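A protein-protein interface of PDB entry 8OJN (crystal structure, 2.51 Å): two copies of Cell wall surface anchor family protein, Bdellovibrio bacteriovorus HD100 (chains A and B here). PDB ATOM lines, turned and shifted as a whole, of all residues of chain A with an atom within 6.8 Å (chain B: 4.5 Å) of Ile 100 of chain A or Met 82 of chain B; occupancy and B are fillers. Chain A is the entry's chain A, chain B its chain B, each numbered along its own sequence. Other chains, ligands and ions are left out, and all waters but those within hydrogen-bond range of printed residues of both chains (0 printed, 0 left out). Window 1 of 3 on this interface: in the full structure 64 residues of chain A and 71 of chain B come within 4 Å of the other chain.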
ATOM      1  N   LEU A  70     -14.532 -17.372  11.117  1.00  0.00           N
ATOM      2  CA  LEU A  70     -13.372 -17.035  10.309  1.00  0.00           C
ATOM      3  C   LEU A  70     -12.283 -16.602  11.278  1.00  0.00           C
ATOM      4  O   LEU A  70     -12.478 -15.651  12.043  1.00  0.00           O
ATOM      5  CB  LEU A  70     -13.700 -15.927   9.311  1.00  0.00           C
ATOM      6  CG  LEU A  70     -12.518 -15.359   8.522  1.00  0.00           C
ATOM      7  CD1 LEU A  70     -11.890 -16.450   7.655  1.00  0.00           C
ATOM      8  CD2 LEU A  70     -12.931 -14.146   7.679  1.00  0.00           C
ATOM      9  N   TYR A  72      -8.399 -15.457  11.997  1.00  0.00           N
ATOM     10  CA  TYR A  72      -7.131 -14.903  11.541  1.00  0.00           C
ATOM     11  C   TYR A  72      -6.045 -15.250  12.554  1.00  0.00           C
ATOM     12  O   TYR A  72      -6.140 -14.854  13.729  1.00  0.00           O
ATOM     13  CB  TYR A  72      -7.217 -13.387  11.389  1.00  0.00           C
ATOM     14  CG  TYR A  72      -8.184 -12.865  10.354  1.00  0.00           C
ATOM     15  CD1 TYR A  72      -9.510 -12.612  10.682  1.00  0.00           C
ATOM     16  CD2 TYR A  72      -7.760 -12.579   9.060  1.00  0.00           C
ATOM     17  CE1 TYR A  72     -10.394 -12.109   9.744  1.00  0.00           C
ATOM     18  CE2 TYR A  72      -8.637 -12.076   8.117  1.00  0.00           C
ATOM     19  CZ  TYR A  72      -9.952 -11.843   8.467  1.00  0.00           C
ATOM     20  OH  TYR A  72     -10.833 -11.345   7.539  1.00  0.00           O
ATOM     21  N   TRP A  80      -7.297 -12.704  15.497  1.00  0.00           N
ATOM     22  CA  TRP A  80      -8.643 -12.141  15.408  1.00  0.00           C
ATOM     23  C   TRP A  80      -9.619 -13.219  14.964  1.00  0.00           C
ATOM     24  O   TRP A  80      -9.228 -14.273  14.460  1.00  0.00           O
ATOM     25  CB  TRP A  80      -8.702 -10.951  14.436  1.00  0.00           C
ATOM     26  CG  TRP A  80      -8.073  -9.703  14.965  1.00  0.00           C
ATOM     27  CD1 TRP A  80      -6.779  -9.295  14.792  1.00  0.00           C
ATOM     28  CD2 TRP A  80      -8.709  -8.694  15.758  1.00  0.00           C
ATOM     29  NE1 TRP A  80      -6.570  -8.093  15.433  1.00  0.00           N
ATOM     30  CE2 TRP A  80      -7.740  -7.704  16.033  1.00  0.00           C
ATOM     31  CE3 TRP A  80     -10.002  -8.533  16.268  1.00  0.00           C
ATOM     32  CZ2 TRP A  80      -8.026  -6.572  16.790  1.00  0.00           C
ATOM     33  CZ3 TRP A  80     -10.284  -7.408  17.019  1.00  0.00           C
ATOM     34  CH2 TRP A  80      -9.297  -6.443  17.275  1.00  0.00           C
ATOM     35  N   SER A  81     -10.909 -12.944  15.135  1.00  0.00           N
ATOM     36  CA  SER A  81     -11.903 -13.852  14.580  1.00  0.00           C
ATOM     37  C   SER A  81     -13.233 -13.132  14.410  1.00  0.00           C
ATOM     38  O   SER A  81     -13.584 -12.271  15.216  1.00  0.00           O
ATOM     39  CB  SER A  81     -12.077 -15.091  15.465  1.00  0.00           C
ATOM     40  OG  SER A  81     -13.205 -14.950  16.303  1.00  0.00           O
ATOM     41  N   MET A  82     -13.953 -13.484  13.345  1.00  0.00           N
ATOM     42  CA  MET A  82     -15.330 -13.049  13.126  1.00  0.00           C
ATOM     43  C   MET A  82     -16.219 -14.281  13.044  1.00  0.00           C
ATOM     44  O   MET A  82     -16.030 -15.124  12.161  1.00  0.00           O
ATOM     45  CB  MET A  82     -15.459 -12.221  11.849  1.00  0.00           C
ATOM     46  CG  MET A  82     -16.888 -11.783  11.572  1.00  0.00           C
ATOM     47  SD  MET A  82     -16.992 -10.372  10.460  1.00  0.00           S
ATOM     48  CE  MET A  82     -16.698 -11.170   8.886  1.00  0.00           C
ATOM     49  N   MET A  83     -17.188 -14.387  13.954  1.00  0.00           N
ATOM     50  CA  MET A  83     -17.964 -15.612  14.088  1.00  0.00           C
ATOM     51  C   MET A  83     -19.417 -15.299  14.423  1.00  0.00           C
ATOM     52  O   MET A  83     -19.781 -14.168  14.751  1.00  0.00           O
ATOM     53  CB  MET A  83     -17.364 -16.522  15.164  1.00  0.00           C
ATOM     54  CG  MET A  83     -17.521 -15.981  16.581  1.00  0.00           C
ATOM     55  SD  MET A  83     -17.163 -17.228  17.845  1.00  0.00           S
ATOM     56  CE  MET A  83     -18.082 -16.592  19.250  1.00  0.00           C
ATOM     57  N   LEU A  98     -23.477 -11.769  15.608  1.00  0.00           N
ATOM     58  CA  LEU A  98     -22.181 -11.695  14.946  1.00  0.00           C
ATOM     59  C   LEU A  98     -21.184 -11.021  15.873  1.00  0.00           C
ATOM     60  O   LEU A  98     -21.370  -9.862  16.245  1.00  0.00           O
ATOM     61  CB  LEU A  98     -22.271 -10.933  13.629  1.00  0.00           C
ATOM     62  CG  LEU A  98     -20.942 -10.873  12.878  1.00  0.00           C
ATOM     63  CD1 LEU A  98     -20.713 -12.172  12.125  1.00  0.00           C
ATOM     64  CD2 LEU A  98     -20.905  -9.683  11.934  1.00  0.00           C
ATOM     65  N   SER A  99     -20.122 -11.735  16.230  1.00  0.00           N
ATOM     66  CA  SER A  99     -19.121 -11.234  17.158  1.00  0.00           C
ATOM     67  C   SER A  99     -17.758 -11.182  16.480  1.00  0.00           C
ATOM     68  O   SER A  99     -17.362 -12.125  15.782  1.00  0.00           O
ATOM     69  CB  SER A  99     -19.061 -12.103  18.417  1.00  0.00           C
ATOM     70  OG  SER A  99     -19.956 -11.635  19.416  1.00  0.00           O
ATOM     71  N   ILE A 100     -17.057 -10.070  16.672  1.00  0.00           N
ATOM     72  CA  ILE A 100     -15.654  -9.930  16.309  1.00  0.00           C
ATOM     73  C   ILE A 100     -14.859  -9.939  17.602  1.00  0.00           C
ATOM     74  O   ILE A 100     -15.095  -9.101  18.491  1.00  0.00           O
ATOM     75  CB  ILE A 100     -15.388  -8.650  15.505  1.00  0.00           C
ATOM     76  CG1 ILE A 100     -16.121  -8.695  14.164  1.00  0.00           C
ATOM     77  CG2 ILE A 100     -13.890  -8.460  15.283  1.00  0.00           C
ATOM     78  CD1 ILE A 100     -15.784  -7.526  13.263  1.00  0.00           C
ATOM     79  N   LEU A 101     -13.914 -10.885  17.683  1.00  0.00           N
ATOM     80  CA  LEU A 101     -13.135 -11.218  18.863  1.00  0.00           C
ATOM     81  C   LEU A 101     -11.652 -10.970  18.608  1.00  0.00           C
ATOM     82  O   LEU A 101     -11.147 -11.193  17.498  1.00  0.00           O
ATOM     83  CB  LEU A 101     -13.317 -12.699  19.258  1.00  0.00           C
ATOM     84  CG  LEU A 101     -14.551 -13.203  20.013  1.00  0.00           C
ATOM     85  CD1 LEU A 101     -15.805 -13.030  19.189  1.00  0.00           C
ATOM     86  CD2 LEU A 101     -14.371 -14.671  20.395  1.00  0.00           C
ATOM     87  N   ARG A 102     -10.958 -10.543  19.664  1.00  0.00           N
ATOM     88  CA  ARG A 102      -9.525 -10.296  19.658  1.00  0.00           C
ATOM     89  C   ARG A 102      -8.848 -11.212  20.668  1.00  0.00           C
ATOM     90  O   ARG A 102      -9.434 -11.568  21.694  1.00  0.00           O
ATOM     91  CB  ARG A 102      -9.211  -8.834  19.998  1.00  0.00           C
ATOM     92  CG  ARG A 102     -10.172  -8.213  21.008  1.00  0.00           C
ATOM     93  CD  ARG A 102      -9.547  -7.009  21.700  1.00  0.00           C
ATOM     94  NE  ARG A 102     -10.278  -6.627  22.906  1.00  0.00           N
ATOM     95  CZ  ARG A 102      -9.705  -6.211  24.034  1.00  0.00           C
ATOM     96  NH1 ARG A 102      -8.384  -6.120  24.122  1.00  0.00           N
ATOM     97  NH2 ARG A 102     -10.452  -5.884  25.079  1.00  0.00           N
ATOM     98  N   GLY A 111     -11.758 -11.049  24.324  1.00  0.00           N
ATOM     99  CA  GLY A 111     -13.164 -10.708  24.375  1.00  0.00           C
ATOM    100  C   GLY A 111     -13.696 -10.272  23.022  1.00  0.00           C
ATOM    101  O   GLY A 111     -12.961 -10.077  22.055  1.00  0.00           O
ATOM    102  N   ALA A 112     -15.016 -10.119  22.985  1.00  0.00           N
ATOM    103  CA  ALA A 112     -15.711  -9.687  21.777  1.00  0.00           C
ATOM    104  C   ALA A 112     -15.580  -8.174  21.668  1.00  0.00           C
ATOM    105  O   ALA A 112     -16.278  -7.426  22.356  1.00  0.00           O
ATOM    106  CB  ALA A 112     -17.172 -10.118  21.812  1.00  0.00           C
ATOM    107  N   ALA A 113     -14.670  -7.716  20.804  1.00  0.00           N
ATOM    108  CA  ALA A 113     -14.543  -6.282  20.574  1.00  0.00           C
ATOM    109  C   ALA A 113     -15.825  -5.703  20.001  1.00  0.00           C
ATOM    110  O   ALA A 113     -16.174  -4.556  20.305  1.00  0.00           O
ATOM    111  CB  ALA A 113     -13.369  -5.988  19.641  1.00  0.00           C
ATOM    112  N   VAL A 114     -16.549  -6.472  19.187  1.00  0.00           N
ATOM    113  CA  VAL A 114     -17.778  -5.971  18.575  1.00  0.00           C
ATOM    114  C   VAL A 114     -18.822  -7.082  18.565  1.00  0.00           C
ATOM    115  O   VAL A 114     -18.496  -8.248  18.324  1.00  0.00           O
ATOM    116  CB  VAL A 114     -17.516  -5.436  17.149  1.00  0.00           C
ATOM    117  CG1 VAL A 114     -18.802  -5.392  16.319  1.00  0.00           C
ATOM    118  CG2 VAL A 114     -16.862  -4.055  17.209  1.00  0.00           C
ATOM    119  N   THR A 115     -20.079  -6.721  18.828  1.00  0.00           N
ATOM    120  CA  THR A 115     -21.177  -7.683  18.776  1.00  0.00           C
ATOM    121  C   THR A 115     -22.403  -7.035  18.151  1.00  0.00           C
ATOM    122  O   THR A 115     -22.864  -5.993  18.620  1.00  0.00           O
ATOM    123  CB  THR A 115     -21.525  -8.213  20.177  1.00  0.00           C
ATOM    124  OG1 THR A 115     -20.386  -8.878  20.745  1.00  0.00           O
ATOM    125  CG2 THR A 115     -22.697  -9.186  20.103  1.00  0.00           C
ATOM    126  N   ILE A 116     -22.942  -7.658  17.107  1.00  0.00           N
ATOM    127  CA  ILE A 116     -24.155  -7.195  16.442  1.00  0.00           C
ATOM    128  C   ILE A 116     -25.269  -8.198  16.700  1.00  0.00           C
ATOM    129  O   ILE A 116     -25.113  -9.396  16.422  1.00  0.00           O
ATOM    130  CB  ILE A 116     -23.939  -7.002  14.934  1.00  0.00           C
ATOM    131  CG1 ILE A 116     -22.567  -6.381  14.671  1.00  0.00           C
ATOM    132  CG2 ILE A 116     -25.038  -6.130  14.366  1.00  0.00           C
ATOM    133  CD1 ILE A 116     -22.354  -6.000  13.233  1.00  0.00           C
ATOM    134  N   SER B  69      -5.270 -12.078   5.304  1.00  0.00           N
ATOM    135  CA  SER B  69      -6.273 -11.171   4.767  1.00  0.00           C
ATOM    136  C   SER B  69      -7.388 -11.945   4.083  1.00  0.00           C
ATOM    137  O   SER B  69      -7.163 -13.009   3.498  1.00  0.00           O
ATOM    138  CB  SER B  69      -5.652 -10.191   3.763  1.00  0.00           C
ATOM    139  OG  SER B  69      -4.377  -9.760   4.204  1.00  0.00           O
ATOM    140  N   LEU B  70      -8.595 -11.388   4.160  1.00  0.00           N
ATOM    141  CA  LEU B  70      -9.736 -11.801   3.351  1.00  0.00           C
ATOM    142  C   LEU B  70     -10.012 -10.654   2.390  1.00  0.00           C
ATOM    143  O   LEU B  70     -10.383  -9.556   2.821  1.00  0.00           O
ATOM    144  CB  LEU B  70     -10.950 -12.103   4.223  1.00  0.00           C
ATOM    145  CG  LEU B  70     -12.290 -12.299   3.516  1.00  0.00           C
ATOM    146  CD1 LEU B  70     -12.378 -13.703   2.952  1.00  0.00           C
ATOM    147  CD2 LEU B  70     -13.447 -12.026   4.473  1.00  0.00           C
ATOM    148  N   SER B  81     -11.340  -5.256   1.960  1.00  0.00           N
ATOM    149  CA  SER B  81     -10.382  -6.111   2.650  1.00  0.00           C
ATOM    150  C   SER B  81     -10.699  -6.158   4.135  1.00  0.00           C
ATOM    151  O   SER B  81     -11.000  -5.127   4.738  1.00  0.00           O
ATOM    152  CB  SER B  81      -8.953  -5.595   2.459  1.00  0.00           C
ATOM    153  OG  SER B  81      -8.004  -6.623   2.639  1.00  0.00           O
ATOM    154  N   MET B  82     -10.610  -7.349   4.725  1.00  0.00           N
ATOM    155  CA  MET B  82     -10.573  -7.486   6.178  1.00  0.00           C
ATOM    156  C   MET B  82      -9.320  -8.269   6.531  1.00  0.00           C
ATOM    157  O   MET B  82      -9.202  -9.447   6.180  1.00  0.00           O
ATOM    158  CB  MET B  82     -11.817  -8.176   6.729  1.00  0.00           C
ATOM    159  CG  MET B  82     -11.767  -8.288   8.244  1.00  0.00           C
ATOM    160  SD  MET B  82     -13.244  -8.980   8.986  1.00  0.00           S
ATOM    161  CE  MET B  82     -13.871  -7.563   9.873  1.00  0.00           C
ATOM    162  N   MET B  83      -8.387  -7.625   7.229  1.00  0.00           N
ATOM    163  CA  MET B  83      -7.068  -8.213   7.393  1.00  0.00           C
ATOM    164  C   MET B  83      -6.452  -7.797   8.718  1.00  0.00           C
ATOM    165  O   MET B  83      -6.825  -6.787   9.321  1.00  0.00           O
ATOM    166  CB  MET B  83      -6.144  -7.801   6.250  1.00  0.00           C
ATOM    167  CG  MET B  83      -5.923  -6.305   6.160  1.00  0.00           C
ATOM    168  SD  MET B  83      -4.628  -5.917   4.973  1.00  0.00           S
ATOM    169  CE  MET B  83      -3.221  -6.740   5.705  1.00  0.00           C
ATOM    170  N   LEU B  98      -6.910  -5.192  13.716  1.00  0.00           N
ATOM    171  CA  LEU B  98      -7.843  -5.607  12.676  1.00  0.00           C
ATOM    172  C   LEU B  98      -8.224  -4.410  11.820  1.00  0.00           C
ATOM    173  O   LEU B  98      -8.463  -3.318  12.339  1.00  0.00           O
ATOM    174  CB  LEU B  98      -9.102  -6.235  13.269  1.00  0.00           C
ATOM    175  CG  LEU B  98     -10.017  -6.935  12.262  1.00  0.00           C
ATOM    176  CD1 LEU B  98      -9.371  -8.213  11.759  1.00  0.00           C
ATOM    177  CD2 LEU B  98     -11.367  -7.224  12.881  1.00  0.00           C
ATOM    178  N   SER B  99      -8.294  -4.617  10.509  1.00  0.00           N
ATOM    179  CA  SER B  99      -8.520  -3.516   9.589  1.00  0.00           C
ATOM    180  C   SER B  99      -9.519  -3.929   8.522  1.00  0.00           C
ATOM    181  O   SER B  99      -9.371  -4.985   7.901  1.00  0.00           O
ATOM    182  CB  SER B  99      -7.209  -3.071   8.932  1.00  0.00           C
ATOM    183  OG  SER B  99      -6.607  -2.014   9.657  1.00  0.00           O
ATOM    184  N   ILE B 100     -10.536  -3.101   8.329  1.00  0.00           N
ATOM    185  CA  ILE B 100     -11.366  -3.136   7.136  1.00  0.00           C
ATOM    186  C   ILE B 100     -10.902  -1.998   6.239  1.00  0.00           C
ATOM    187  O   ILE B 100     -11.078  -0.818   6.577  1.00  0.00           O
ATOM    188  CB  ILE B 100     -12.855  -3.009   7.468  1.00  0.00           C
ATOM    189  CG1 ILE B 100     -13.325  -4.239   8.243  1.00  0.00           C
ATOM    190  CG2 ILE B 100     -13.646  -2.840   6.187  1.00  0.00           C
ATOM    191  CD1 ILE B 100     -14.760  -4.151   8.720  1.00  0.00           C
ATOM    192  N   ILE B 116      -9.570  -1.898  14.554  1.00  0.00           N
ATOM    193  CA  ILE B 116      -9.814  -2.315  15.929  1.00  0.00           C
ATOM    194  C   ILE B 116      -8.480  -2.671  16.563  1.00  0.00           C
ATOM    195  O   ILE B 116      -7.733  -3.508  16.032  1.00  0.00           O
ATOM    196  CB  ILE B 116     -10.798  -3.490  16.012  1.00  0.00           C
ATOM    197  CG1 ILE B 116     -11.953  -3.281  15.040  1.00  0.00           C
ATOM    198  CG2 ILE B 116     -11.342  -3.612  17.424  1.00  0.00           C
ATOM    199  CD1 ILE B 116     -12.935  -4.428  15.019  1.00  0.00           C
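The backbone carbonyl oxygen (O) of Met 82 of chain B lies within hydrogen-bond range of the side-chain hydroxyl (OH) of Tyr 72 of chain A (2.8 Å).
The backbone NH (N) of Leu 98 of chain B lies close to the indole nitrogen (NE1) of Trp 80 of chain A, 3.4 Å away.
N of Leu 70 of chain B lies within hydrogen-bond range of O of Met 82 of chain B (2.9 Å).
The backbone carbonyl oxygen (O) of Leu 98 of chain B lies within hydrogen-bond range of the backbone NH (N) of Ile 116 of chain B (2.9 Å).
N of Leu 70 of chain A sits at hydrogen-bond distance from O of Met 82 of chain A (2.9 Å).
The backbone carbonyl oxygen (O) of Trp 80 of chain A sits at hydrogen-bond distance from the backbone NH (N) of Tyr 72 of chain A, at 2.9 Å.
The backbone carbonyl oxygen (O) of Ile 100 of chain A is in hydrogen-bond range of the backbone NH (N) of Ala 113 of chain A (2.7 Å).
The backbone carbonyl oxygen (O) of Val 114 of chain A lies within hydrogen-bond range of the backbone NH (N) of Ile 100 of chain A (2.8 Å).
Leu 70 of chain A touches Leu 70 of chain B (CD2 to CD2, 3.9 Å).
Tyr 72 of chain A touches Leu 70 of chain B (OH to CB, 3.4 Å).
Trp 80 of chain A touches Ile 116 of chain B.
Met 82 of chain B touches Ile 100 of chain A (CE to CD1, 3.9 Å).
Ile 100 of chain A touches Leu 98 of chain B (CG2 to CD2, 3.7 Å).
Ile 116 of chain B touches Ala 113 of chain A (CG2 to CB, 3.8 Å).
Ile 100 of chain A touches just these residues of chain B: Met 82 and Leu 98.
Of chain A, only Tyr 72 and Ile 100 come within 4 Å of Met 82 of chain B.
Of the printed residues of chain A, Leu 98 of chain B touches Trp 80 (3.4 Å) and Ile 100 (3.7 Å).
Of the printed residues of chain B, Tyr 72 of chain A touches Leu 70 (3.4 Å) and Met 82 (2.8 Å).
Ala 112 of chain A touches none of the printed residues of chain B.
Printed residues of chain B that touch a printed residue of chain A: Leu 70, Met 82, Leu 98 and Ile 116.
Hydrophobic or aromatic side chains of chain B that line the printed part of chain A: Leu 70, Met 82, Leu 98 and Ile 116.
Among the printed residues, no Asp or Glu carboxylate lies within 4 Å of a Lys or Arg side-chain nitrogen of the other chain.
Leu 70 of chain A touches its own counterpart, Leu 70 of chain B.
Ile 100 of chain A touches Met 82 of chain B, but with the chains exchanged Met 82 of chain A does not touch Ile 100 of chain B (6.8 Å).
Ile 100 of chain A touches Leu 98 of chain B, but with the chains exchanged Leu 98 of chain A does not touch Ile 100 of chain B (8.9 Å).
Of the 8 pairs that touch across the chains among the printed residues, 1 has its exchanged pair printed and touching as well.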
